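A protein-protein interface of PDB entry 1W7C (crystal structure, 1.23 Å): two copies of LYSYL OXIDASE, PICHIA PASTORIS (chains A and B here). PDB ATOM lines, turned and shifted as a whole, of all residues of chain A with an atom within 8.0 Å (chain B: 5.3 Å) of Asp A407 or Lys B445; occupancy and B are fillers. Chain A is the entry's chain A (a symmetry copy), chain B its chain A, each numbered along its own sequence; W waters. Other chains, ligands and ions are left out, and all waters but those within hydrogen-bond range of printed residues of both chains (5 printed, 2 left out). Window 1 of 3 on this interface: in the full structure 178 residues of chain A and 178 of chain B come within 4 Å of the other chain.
Water W3 lies within hydrogen-bond range of OD2 of Asp A407 (2.5 Å) and OE2 of Glu B406 (2.8 Å). Water W5 bridges the side-chain amide oxygen (OD1) of Asn B404 (2.7 Å) and the backbone carbonyl oxygen (O) of Gln A405 (2.8 Å). Water W4 lies within hydrogen-bond range of the side-chain carboxylate (OD1) of Asp B374 and the side-chain hydroxyl (OG) of Ser A409. Water W2 bridges the backbone carbonyl oxygen (O) of Asp B374 (2.9 Å) and the backbone NH (N) of Ser A409 (3.0 Å). Water W1 lies within hydrogen-bond range of the backbone carbonyl oxygen of Asp A407 (3.3 Å) and the backbone carbonyl oxygen of Asp B374 (3.4 Å).
NH1 of Arg B430 lies within hydrogen-bond range of O of Asp B374 (3.0 Å). The backbone NH (N) of Asn B428 sits at hydrogen-bond distance from the backbone carbonyl oxygen (O) of Phe B402 (2.8 Å). The side-chain carboxylate (OE1) of Glu B406 sits at hydrogen-bond distance from the side-chain amide nitrogen (ND2) of Asn B404 (3.1 Å). N of Asn B404 lies close to ND2 of Asn B428, at 3.5 Å. The side-chain carboxylate (OE1) of Glu B406 lies within salt-bridge range of the side-chain amino group (NZ) of Lys B445 (2.8 Å). The side-chain amide nitrogen (ND2) of Asn A424 sits close to the side-chain hydroxyl (OH) of Tyr A408 (3.2 Å).
Hydrophobic or aromatic side chains of chain B within 4 Å of the printed part of chain A: Phe B402 and Leu B443. Of the 9 printed residues of chain A, 2 touch a printed residue of chain B. Printed residues of chain A that touch a printed residue of chain B: Asp A407 and Tyr A408. Among the printed residues, 6 pairs touch across the chains.
The side-chain carboxylate of Asp A407 lies within salt-bridge range of the guanidinium group of Arg B430 (3.9 Å). The side-chain carboxylate (OD2) of Asp A407 lies within salt-bridge range of the side-chain amino group (NZ) of Lys B445.
Positions printed for both chains: 404 and 406. Of the 6 pairs that touch across the chains among the printed residues, none has its exchanged pair printed and touching as well.
Among the printed residues, merely in contact across the chains: Tyr A408 with Arg B430, Asp A407 with Asn B404, Asp A407 with Leu B443 and Asp A407 with Phe B402.
Of the printed residues of chain B, Asp A407 touches Phe B402 (3.997 Å), Asn B404 (3.8 Å), Arg B430 (2.8 Å), Leu B443 (3.9 Å) and Lys B445 (2.8 Å). Lys B445 touches one residue of chain A. Printed residues of chain A within 4 Å of Arg B430: Asp A407 (2.8 Å) and Tyr A408 (3.4 Å). Printed residues of chain A within 4 Å of Asn B404: Asp A407 (3.8 Å). Of the printed residues of chain A, Leu B443 touches Asp A407 (3.9 Å). Of the printed residues of chain A, Phe B402 touches Asp A407 (3.997 Å). The nearest printed residue of chain B that does not touch Asp A407 is Asn B428 (4.4 Å). The nearest printed residue of chain A that does not touch Arg B430 is Ser A409 (5.5 Å).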
ATOM      1  N   ASN A 404      -2.722 -12.240  30.752  1.00  0.00           N
ATOM      2  CA  ASN A 404      -3.903 -11.463  30.398  1.00  0.00           C
ATOM      3  C   ASN A 404      -5.146 -12.072  31.017  1.00  0.00           C
ATOM      4  O   ASN A 404      -5.155 -13.261  31.326  1.00  0.00           O
ATOM      5  CB  ASN A 404      -4.087 -11.369  28.868  1.00  0.00           C
ATOM      6  CG  ASN A 404      -5.042 -10.268  28.461  1.00  0.00           C
ATOM      7  OD1 ASN A 404      -5.132  -9.217  29.143  1.00  0.00           O
ATOM      8  ND2 ASN A 404      -5.761 -10.465  27.338  1.00  0.00           N
ATOM      9  N   GLN A 405      -6.190 -11.246  31.183  1.00  0.00           N
ATOM     10  CA  GLN A 405      -7.553 -11.745  31.381  1.00  0.00           C
ATOM     11  C   GLN A 405      -8.255 -11.484  30.071  1.00  0.00           C
ATOM     12  O   GLN A 405      -8.531 -10.344  29.693  1.00  0.00           O
ATOM     13  CB  GLN A 405      -8.236 -11.010  32.532  1.00  0.00           C
ATOM     14  CG  GLN A 405      -9.605 -11.612  32.899  1.00  0.00           C
ATOM     15  CD  GLN A 405      -9.521 -12.999  33.485  1.00  0.00           C
ATOM     16  OE1 GLN A 405     -10.064 -13.953  32.920  1.00  0.00           O
ATOM     17  NE2 GLN A 405      -8.912 -13.104  34.678  1.00  0.00           N
ATOM     18  N   GLU A 406      -8.559 -12.534  29.327  1.00  0.00           N
ATOM     19  CA  GLU A 406      -9.225 -12.330  28.066  1.00  0.00           C
ATOM     20  C   GLU A 406     -10.634 -11.782  28.294  1.00  0.00           C
ATOM     21  O   GLU A 406     -11.216 -11.987  29.345  1.00  0.00           O
ATOM     22  CB  GLU A 406      -9.310 -13.626  27.256  1.00  0.00           C
ATOM     23  CG  GLU A 406      -7.983 -14.283  26.912  1.00  0.00           C
ATOM     24  CD  GLU A 406      -7.072 -13.443  26.064  1.00  0.00           C
ATOM     25  OE1 GLU A 406      -5.867 -13.359  26.377  1.00  0.00           O
ATOM     26  OE2 GLU A 406      -7.565 -12.909  25.033  1.00  0.00           O
ATOM     27  N   ASP A 407     -11.184 -11.107  27.266  1.00  0.00           N
ATOM     28  CA  ASP A 407     -12.445 -10.387  27.376  1.00  0.00           C
ATOM     29  C   ASP A 407     -13.691 -11.276  27.326  1.00  0.00           C
ATOM     30  O   ASP A 407     -14.792 -10.773  27.397  1.00  0.00           O
ATOM     31  CB  ASP A 407     -12.535  -9.269  26.317  1.00  0.00           C
ATOM     32  CG  ASP A 407     -12.689  -9.783  24.872  1.00  0.00           C
ATOM     33  OD1 ASP A 407     -13.099 -10.923  24.645  1.00  0.00           O
ATOM     34  OD2 ASP A 407     -12.435  -9.062  23.871  1.00  0.00           O
ATOM     35  N   TYR A 408     -13.486 -12.575  27.257  1.00  0.00           N
ATOM     36  CA  TYR A 408     -14.554 -13.583  27.213  1.00  0.00           C
ATOM     37  C   TYR A 408     -14.095 -14.752  28.104  1.00  0.00           C
ATOM     38  O   TYR A 408     -12.880 -15.036  28.217  1.00  0.00           O
ATOM     39  CB  TYR A 408     -14.821 -14.054  25.767  1.00  0.00           C
ATOM     40  CG  TYR A 408     -13.650 -14.780  25.188  1.00  0.00           C
ATOM     41  CD1 TYR A 408     -12.549 -14.098  24.694  1.00  0.00           C
ATOM     42  CD2 TYR A 408     -13.630 -16.166  25.131  1.00  0.00           C
ATOM     43  CE1 TYR A 408     -11.449 -14.773  24.172  1.00  0.00           C
ATOM     44  CE2 TYR A 408     -12.551 -16.845  24.604  1.00  0.00           C
ATOM     45  CZ  TYR A 408     -11.456 -16.158  24.139  1.00  0.00           C
ATOM     46  OH  TYR A 408     -10.363 -16.868  23.714  1.00  0.00           O
ATOM     47  N   SER A 409     -15.061 -15.411  28.717  1.00  0.00           N
ATOM     48  CA  SER A 409     -14.763 -16.563  29.550  1.00  0.00           C
ATOM     49  C   SER A 409     -14.288 -17.761  28.714  1.00  0.00           C
ATOM     50  O   SER A 409     -14.527 -17.822  27.510  1.00  0.00           O
ATOM     51  CB  SER A 409     -15.969 -16.884  30.477  1.00  0.00           C
ATOM     52  OG  SER A 409     -16.838 -17.776  29.832  1.00  0.00           O
ATOM     53  N   LEU A 410     -13.584 -18.705  29.333  1.00  0.00           N
ATOM     54  CA  LEU A 410     -13.086 -19.851  28.568  1.00  0.00           C
ATOM     55  C   LEU A 410     -14.233 -20.769  28.172  1.00  0.00           C
ATOM     56  O   LEU A 410     -14.233 -21.314  27.081  1.00  0.00           O
ATOM     57  CB  LEU A 410     -11.997 -20.598  29.358  1.00  0.00           C
ATOM     58  CG  LEU A 410     -11.358 -21.790  28.618  1.00  0.00           C
ATOM     59  CD1 LEU A 410     -10.739 -21.376  27.295  1.00  0.00           C
ATOM     60  CD2 LEU A 410     -10.304 -22.383  29.535  1.00  0.00           C
ATOM     61  N   ASN A 424     -10.779 -16.954  31.720  1.00  0.00           N
ATOM     62  CA  ASN A 424      -9.831 -17.206  30.626  1.00  0.00           C
ATOM     63  C   ASN A 424      -8.552 -16.363  30.769  1.00  0.00           C
ATOM     64  O   ASN A 424      -8.257 -15.535  29.940  1.00  0.00           O
ATOM     65  CB  ASN A 424     -10.536 -16.882  29.303  1.00  0.00           C
ATOM     66  CG  ASN A 424      -9.884 -17.453  28.076  1.00  0.00           C
ATOM     67  OD1 ASN A 424      -8.953 -18.264  28.121  1.00  0.00           O
ATOM     68  ND2 ASN A 424     -10.437 -17.060  26.917  1.00  0.00           N
ATOM     69  N   PRO A 425      -7.777 -16.631  31.807  1.00  0.00           N
ATOM     70  CA  PRO A 425      -6.423 -16.069  31.898  1.00  0.00           C
ATOM     71  C   PRO A 425      -5.503 -16.784  30.934  1.00  0.00           C
ATOM     72  O   PRO A 425      -5.619 -17.983  30.731  1.00  0.00           O
ATOM     73  CB  PRO A 425      -6.015 -16.385  33.325  1.00  0.00           C
ATOM     74  CG  PRO A 425      -6.716 -17.699  33.586  1.00  0.00           C
ATOM     75  CD  PRO A 425      -8.069 -17.524  32.946  1.00  0.00           C
ATOM     76  N   ASP B 374     -19.013 -13.391  33.133  1.00  0.00           N
ATOM     77  CA  ASP B 374     -19.491 -13.231  31.771  1.00  0.00           C
ATOM     78  C   ASP B 374     -19.033 -11.911  31.143  1.00  0.00           C
ATOM     79  O   ASP B 374     -18.858 -11.855  29.920  1.00  0.00           O
ATOM     80  CB  ASP B 374     -21.010 -13.335  31.671  1.00  0.00           C
ATOM     81  CG  ASP B 374     -21.532 -14.749  31.753  1.00  0.00           C
ATOM     82  OD1 ASP B 374     -20.804 -15.727  31.455  1.00  0.00           O
ATOM     83  OD2 ASP B 374     -22.717 -14.936  32.130  1.00  0.00           O
ATOM     84  N   PRO B 376     -16.456  -8.310  32.334  1.00  0.00           N
ATOM     85  CA  PRO B 376     -15.596  -7.758  33.394  1.00  0.00           C
ATOM     86  C   PRO B 376     -16.376  -6.976  34.438  1.00  0.00           C
ATOM     87  O   PRO B 376     -17.490  -6.480  34.242  1.00  0.00           O
ATOM     88  CB  PRO B 376     -14.619  -6.848  32.623  1.00  0.00           C
ATOM     89  CG  PRO B 376     -14.682  -7.334  31.205  1.00  0.00           C
ATOM     90  CD  PRO B 376     -16.065  -7.810  31.009  1.00  0.00           C
ATOM     91  N   PHE B 402     -18.806  -2.533  28.322  1.00  0.00           N
ATOM     92  CA  PHE B 402     -17.547  -2.337  29.003  1.00  0.00           C
ATOM     93  C   PHE B 402     -16.457  -1.860  28.071  1.00  0.00           C
ATOM     94  O   PHE B 402     -16.479  -2.131  26.863  1.00  0.00           O
ATOM     95  CB  PHE B 402     -17.071  -3.596  29.767  1.00  0.00           C
ATOM     96  CG  PHE B 402     -16.772  -4.793  28.888  1.00  0.00           C
ATOM     97  CD1 PHE B 402     -17.783  -5.659  28.522  1.00  0.00           C
ATOM     98  CD2 PHE B 402     -15.470  -5.061  28.478  1.00  0.00           C
ATOM     99  CE1 PHE B 402     -17.523  -6.781  27.744  1.00  0.00           C
ATOM    100  CE2 PHE B 402     -15.199  -6.190  27.697  1.00  0.00           C
ATOM    101  CZ  PHE B 402     -16.223  -7.041  27.335  1.00  0.00           C
ATOM    102  N   ASN B 404     -12.666  -2.364  27.199  1.00  0.00           N
ATOM    103  CA  ASN B 404     -11.504  -3.228  27.364  1.00  0.00           C
ATOM    104  C   ASN B 404     -10.227  -2.462  27.083  1.00  0.00           C
ATOM    105  O   ASN B 404     -10.259  -1.458  26.376  1.00  0.00           O
ATOM    106  CB  ASN B 404     -11.576  -4.462  26.439  1.00  0.00           C
ATOM    107  CG  ASN B 404     -10.620  -5.560  26.854  1.00  0.00           C
ATOM    108  OD1 ASN B 404     -10.334  -5.732  28.065  1.00  0.00           O
ATOM    109  ND2 ASN B 404     -10.119  -6.338  25.874  1.00  0.00           N
ATOM    110  N   GLU B 406      -7.196  -3.710  25.090  1.00  0.00           N
ATOM    111  CA  GLU B 406      -6.739  -4.850  24.336  1.00  0.00           C
ATOM    112  C   GLU B 406      -5.273  -5.143  24.656  1.00  0.00           C
ATOM    113  O   GLU B 406      -4.539  -4.260  25.065  1.00  0.00           O
ATOM    114  CB  GLU B 406      -6.894  -4.629  22.830  1.00  0.00           C
ATOM    115  CG  GLU B 406      -8.307  -4.359  22.339  1.00  0.00           C
ATOM    116  CD  GLU B 406      -9.281  -5.475  22.594  1.00  0.00           C
ATOM    117  OE1 GLU B 406     -10.405  -5.198  23.059  1.00  0.00           O
ATOM    118  OE2 GLU B 406      -8.928  -6.640  22.264  1.00  0.00           O
ATOM    119  N   THR B 426     -11.188  -0.377  23.736  1.00  0.00           N
ATOM    120  CA  THR B 426     -12.335  -0.683  22.866  1.00  0.00           C
ATOM    121  C   THR B 426     -13.621  -0.655  23.681  1.00  0.00           C
ATOM    122  O   THR B 426     -13.628  -1.008  24.869  1.00  0.00           O
ATOM    123  CB  THR B 426     -12.220  -2.051  22.190  1.00  0.00           C
ATOM    124  OG1 THR B 426     -12.066  -3.056  23.197  1.00  0.00           O
ATOM    125  CG2 THR B 426     -11.040  -2.083  21.257  1.00  0.00           C
ATOM    126  N   LEU B 427     -14.694  -0.219  23.055  1.00  0.00           N
ATOM    127  CA  LEU B 427     -16.026  -0.396  23.647  1.00  0.00           C
ATOM    128  C   LEU B 427     -16.552  -1.771  23.248  1.00  0.00           C
ATOM    129  O   LEU B 427     -16.408  -2.182  22.118  1.00  0.00           O
ATOM    130  CB  LEU B 427     -17.016   0.661  23.159  1.00  0.00           C
ATOM    131  CG  LEU B 427     -18.349   0.676  23.877  1.00  0.00           C
ATOM    132  CD1 LEU B 427     -18.153   1.203  25.301  1.00  0.00           C
ATOM    133  CD2 LEU B 427     -19.363   1.509  23.156  1.00  0.00           C
ATOM    134  N   ASN B 428     -17.206  -2.435  24.190  1.00  0.00           N
ATOM    135  CA  ASN B 428     -17.670  -3.796  24.009  1.00  0.00           C
ATOM    136  C   ASN B 428     -19.089  -3.898  24.517  1.00  0.00           C
ATOM    137  O   ASN B 428     -19.366  -3.472  25.645  1.00  0.00           O
ATOM    138  CB  ASN B 428     -16.770  -4.747  24.803  1.00  0.00           C
ATOM    139  CG  ASN B 428     -15.369  -4.807  24.262  1.00  0.00           C
ATOM    140  OD1 ASN B 428     -15.108  -5.612  23.348  1.00  0.00           O
ATOM    141  ND2 ASN B 428     -14.491  -3.878  24.686  1.00  0.00           N
ATOM    142  N   VAL B 429     -19.937  -4.474  23.657  1.00  0.00           N
ATOM    143  CA  VAL B 429     -21.335  -4.767  23.992  1.00  0.00           C
ATOM    144  C   VAL B 429     -21.504  -6.282  23.841  1.00  0.00           C
ATOM    145  O   VAL B 429     -21.229  -6.855  22.766  1.00  0.00           O
ATOM    146  CB  VAL B 429     -22.320  -3.998  23.112  1.00  0.00           C
ATOM    147  CG1 VAL B 429     -23.743  -4.251  23.558  1.00  0.00           C
ATOM    148  CG2 VAL B 429     -21.992  -2.490  23.044  1.00  0.00           C
ATOM    149  N   ARG B 430     -21.881  -6.933  24.956  1.00  0.00           N
ATOM    150  CA  ARG B 430     -22.086  -8.381  24.943  1.00  0.00           C
ATOM    151  C   ARG B 430     -23.471  -8.789  25.442  1.00  0.00           C
ATOM    152  O   ARG B 430     -24.017  -8.162  26.363  1.00  0.00           O
ATOM    153  CB  ARG B 430     -21.057  -9.062  25.853  1.00  0.00           C
ATOM    154  CG  ARG B 430     -21.354 -10.491  26.225  1.00  0.00           C
ATOM    155  CD  ARG B 430     -20.237 -11.157  27.028  1.00  0.00           C
ATOM    156  NE  ARG B 430     -19.078 -11.415  26.179  1.00  0.00           N
ATOM    157  CZ  ARG B 430     -17.840 -11.076  26.434  1.00  0.00           C
ATOM    158  NH1 ARG B 430     -17.522 -10.468  27.571  1.00  0.00           N
ATOM    159  NH2 ARG B 430     -16.895 -11.344  25.561  1.00  0.00           N
ATOM    160  N   LEU B 443     -20.475 -10.591  20.810  1.00  0.00           N
ATOM    161  CA  LEU B 443     -19.683  -9.422  21.162  1.00  0.00           C
ATOM    162  C   LEU B 443     -19.624  -8.468  19.967  1.00  0.00           C
ATOM    163  O   LEU B 443     -19.428  -8.881  18.844  1.00  0.00           O
ATOM    164  CB  LEU B 443     -18.276  -9.848  21.594  1.00  0.00           C
ATOM    165  CG  LEU B 443     -17.381  -8.745  22.104  1.00  0.00           C
ATOM    166  CD1 LEU B 443     -17.886  -8.169  23.411  1.00  0.00           C
ATOM    167  CD2 LEU B 443     -15.972  -9.255  22.276  1.00  0.00           C
ATOM    168  N   TYR B 444     -19.753  -7.181  20.272  1.00  0.00           N
ATOM    169  CA  TYR B 444     -19.628  -6.076  19.345  1.00  0.00           C
ATOM    170  C   TYR B 444     -18.541  -5.167  19.949  1.00  0.00           C
ATOM    171  O   TYR B 444     -18.713  -4.650  21.049  1.00  0.00           O
ATOM    172  CB  TYR B 444     -20.978  -5.359  19.183  1.00  0.00           C
ATOM    173  CG  TYR B 444     -22.039  -6.250  18.656  1.00  0.00           C
ATOM    174  CD1 TYR B 444     -22.746  -7.106  19.481  1.00  0.00           C
ATOM    175  CD2 TYR B 444     -22.325  -6.289  17.295  1.00  0.00           C
ATOM    176  CE1 TYR B 444     -23.681  -8.022  18.963  1.00  0.00           C
ATOM    177  CE2 TYR B 444     -23.258  -7.179  16.785  1.00  0.00           C
ATOM    178  CZ  TYR B 444     -23.963  -8.007  17.610  1.00  0.00           C
ATOM    179  OH  TYR B 444     -24.895  -8.857  17.042  1.00  0.00           O
ATOM    180  N   LYS B 445     -17.442  -4.978  19.198  1.00  0.00           N
ATOM    181  CA  LYS B 445     -16.239  -4.327  19.699  1.00  0.00           C
ATOM    182  C   LYS B 445     -15.893  -3.158  18.781  1.00  0.00           C
ATOM    183  O   LYS B 445     -15.688  -3.340  17.571  1.00  0.00           O
ATOM    184  CB  LYS B 445     -15.122  -5.369  19.701  1.00  0.00           C
ATOM    185  CG  LYS B 445     -13.803  -4.808  20.246  1.00  0.00           C
ATOM    186  CD  LYS B 445     -12.643  -5.809  20.099  1.00  0.00           C
ATOM    187  CE  LYS B 445     -12.774  -7.023  21.049  1.00  0.00           C
ATOM    188  NZ  LYS B 445     -12.708  -6.698  22.490  1.00  0.00           N
ATOM    189  N   PHE B 446     -15.867  -1.970  19.348  1.00  0.00           N
ATOM    190  CA  PHE B 446     -15.661  -0.724  18.636  1.00  0.00           C
ATOM    191  C   PHE B 446     -14.263  -0.151  18.933  1.00  0.00           C
ATOM    192  O   PHE B 446     -13.856  -0.151  20.081  1.00  0.00           O
ATOM    193  CB  PHE B 446     -16.706   0.335  19.058  1.00  0.00           C
ATOM    194  CG  PHE B 446     -18.159  -0.080  18.793  1.00  0.00           C
ATOM    195  CD1 PHE B 446     -18.822  -0.949  19.652  1.00  0.00           C
ATOM    196  CD2 PHE B 446     -18.851   0.434  17.730  1.00  0.00           C
ATOM    197  CE1 PHE B 446     -20.139  -1.297  19.443  1.00  0.00           C
ATOM    198  CE2 PHE B 446     -20.160   0.064  17.501  1.00  0.00           C
ATOM    199  CZ  PHE B 446     -20.783  -0.804  18.322  1.00  0.00           C
ATOM    200  N   PHE B 447     -13.581   0.290  17.880  1.00  0.00           N
ATOM    201  CA  PHE B 447     -12.187   0.759  17.967  1.00  0.00           C
ATOM    202  C   PHE B 447     -12.075   2.263  17.731  1.00  0.00           C
ATOM    203  O   PHE B 447     -12.953   2.889  17.099  1.00  0.00           O
ATOM    204  CB  PHE B 447     -11.354   0.036  16.929  1.00  0.00           C
ATOM    205  CG  PHE B 447     -11.197  -1.463  17.163  1.00  0.00           C
ATOM    206  CD1 PHE B 447     -10.036  -1.972  17.727  1.00  0.00           C
ATOM    207  CD2 PHE B 447     -12.210  -2.350  16.803  1.00  0.00           C
ATOM    208  CE1 PHE B 447      -9.877  -3.342  17.886  1.00  0.00           C
ATOM    209  CE2 PHE B 447     -12.052  -3.701  16.962  1.00  0.00           C
ATOM    210  CZ  PHE B 447     -10.872  -4.198  17.512  1.00  0.00           C
ATOM    211  N   THR B 451     -13.289   1.365  13.276  1.00  0.00           N
ATOM    212  CA  THR B 451     -13.523  -0.057  12.955  1.00  0.00           C
ATOM    213  C   THR B 451     -14.457  -0.657  13.971  1.00  0.00           C
ATOM    214  O   THR B 451     -14.358  -0.327  15.139  1.00  0.00           O
ATOM    215  CB  THR B 451     -12.188  -0.809  12.959  1.00  0.00           C
ATOM    216  OG1 THR B 451     -11.376  -0.330  11.871  1.00  0.00           O
ATOM    217  CG2 THR B 451     -12.307  -2.327  12.799  1.00  0.00           C
ATOM    218  N   LEU B 452     -15.314  -1.570  13.560  1.00  0.00           N
ATOM    219  CA  LEU B 452     -16.168  -2.360  14.432  1.00  0.00           C
ATOM    220  C   LEU B 452     -15.952  -3.845  14.101  1.00  0.00           C
ATOM    221  O   LEU B 452     -15.895  -4.209  12.942  1.00  0.00           O
ATOM    222  CB  LEU B 452     -17.650  -1.993  14.156  1.00  0.00           C
ATOM    223  CG  LEU B 452     -18.785  -2.882  14.691  1.00  0.00           C
ATOM    224  CD1 LEU B 452     -18.698  -3.012  16.207  1.00  0.00           C
ATOM    225  CD2 LEU B 452     -20.144  -2.273  14.257  1.00  0.00           C
ATOM    226  N   GLU B 453     -15.882  -4.676  15.135  1.00  0.00           N
ATOM    227  CA  GLU B 453     -15.761  -6.115  14.967  1.00  0.00           C
ATOM    228  C   GLU B 453     -16.992  -6.771  15.599  1.00  0.00           C
ATOM    229  O   GLU B 453     -17.312  -6.484  16.767  1.00  0.00           O
ATOM    230  CB  GLU B 453     -14.498  -6.622  15.666  1.00  0.00           C
ATOM    231  CG  GLU B 453     -14.300  -8.127  15.560  1.00  0.00           C
ATOM    232  CD  GLU B 453     -13.237  -8.632  16.526  1.00  0.00           C
ATOM    233  OE1 GLU B 453     -12.160  -9.001  16.032  1.00  0.00           O
ATOM    234  OE2 GLU B 453     -13.457  -8.623  17.781  1.00  0.00           O
ATOM    235  N   VAL B 454     -17.592  -7.671  14.817  1.00  0.00           N
ATOM    236  CA  VAL B 454     -18.748  -8.456  15.194  1.00  0.00           C
ATOM    237  C   VAL B 454     -18.258  -9.888  15.382  1.00  0.00           C
ATOM    238  O   VAL B 454     -17.643 -10.442  14.469  1.00  0.00           O
ATOM    239  CB  VAL B 454     -19.809  -8.385  14.113  1.00  0.00           C
ATOM    240  CG1 VAL B 454     -20.984  -9.302  14.439  1.00  0.00           C
ATOM    241  CG2 VAL B 454     -20.280  -6.993  13.889  1.00  0.00           C
HETATM  242  O   HOH W   1     -15.580 -11.454  30.580  1.00  0.00           O
HETATM  243  O   HOH W   2     -17.756 -14.037  28.361  1.00  0.00           O
HETATM  244  O   HOH W   3     -10.126  -9.078  22.819  1.00  0.00           O
HETATM  245  O   HOH W   4     -19.069 -16.222  29.373  1.00  0.00           O
HETATM  246  O   HOH W   5     -10.047  -7.990  29.598  1.00  0.00           O
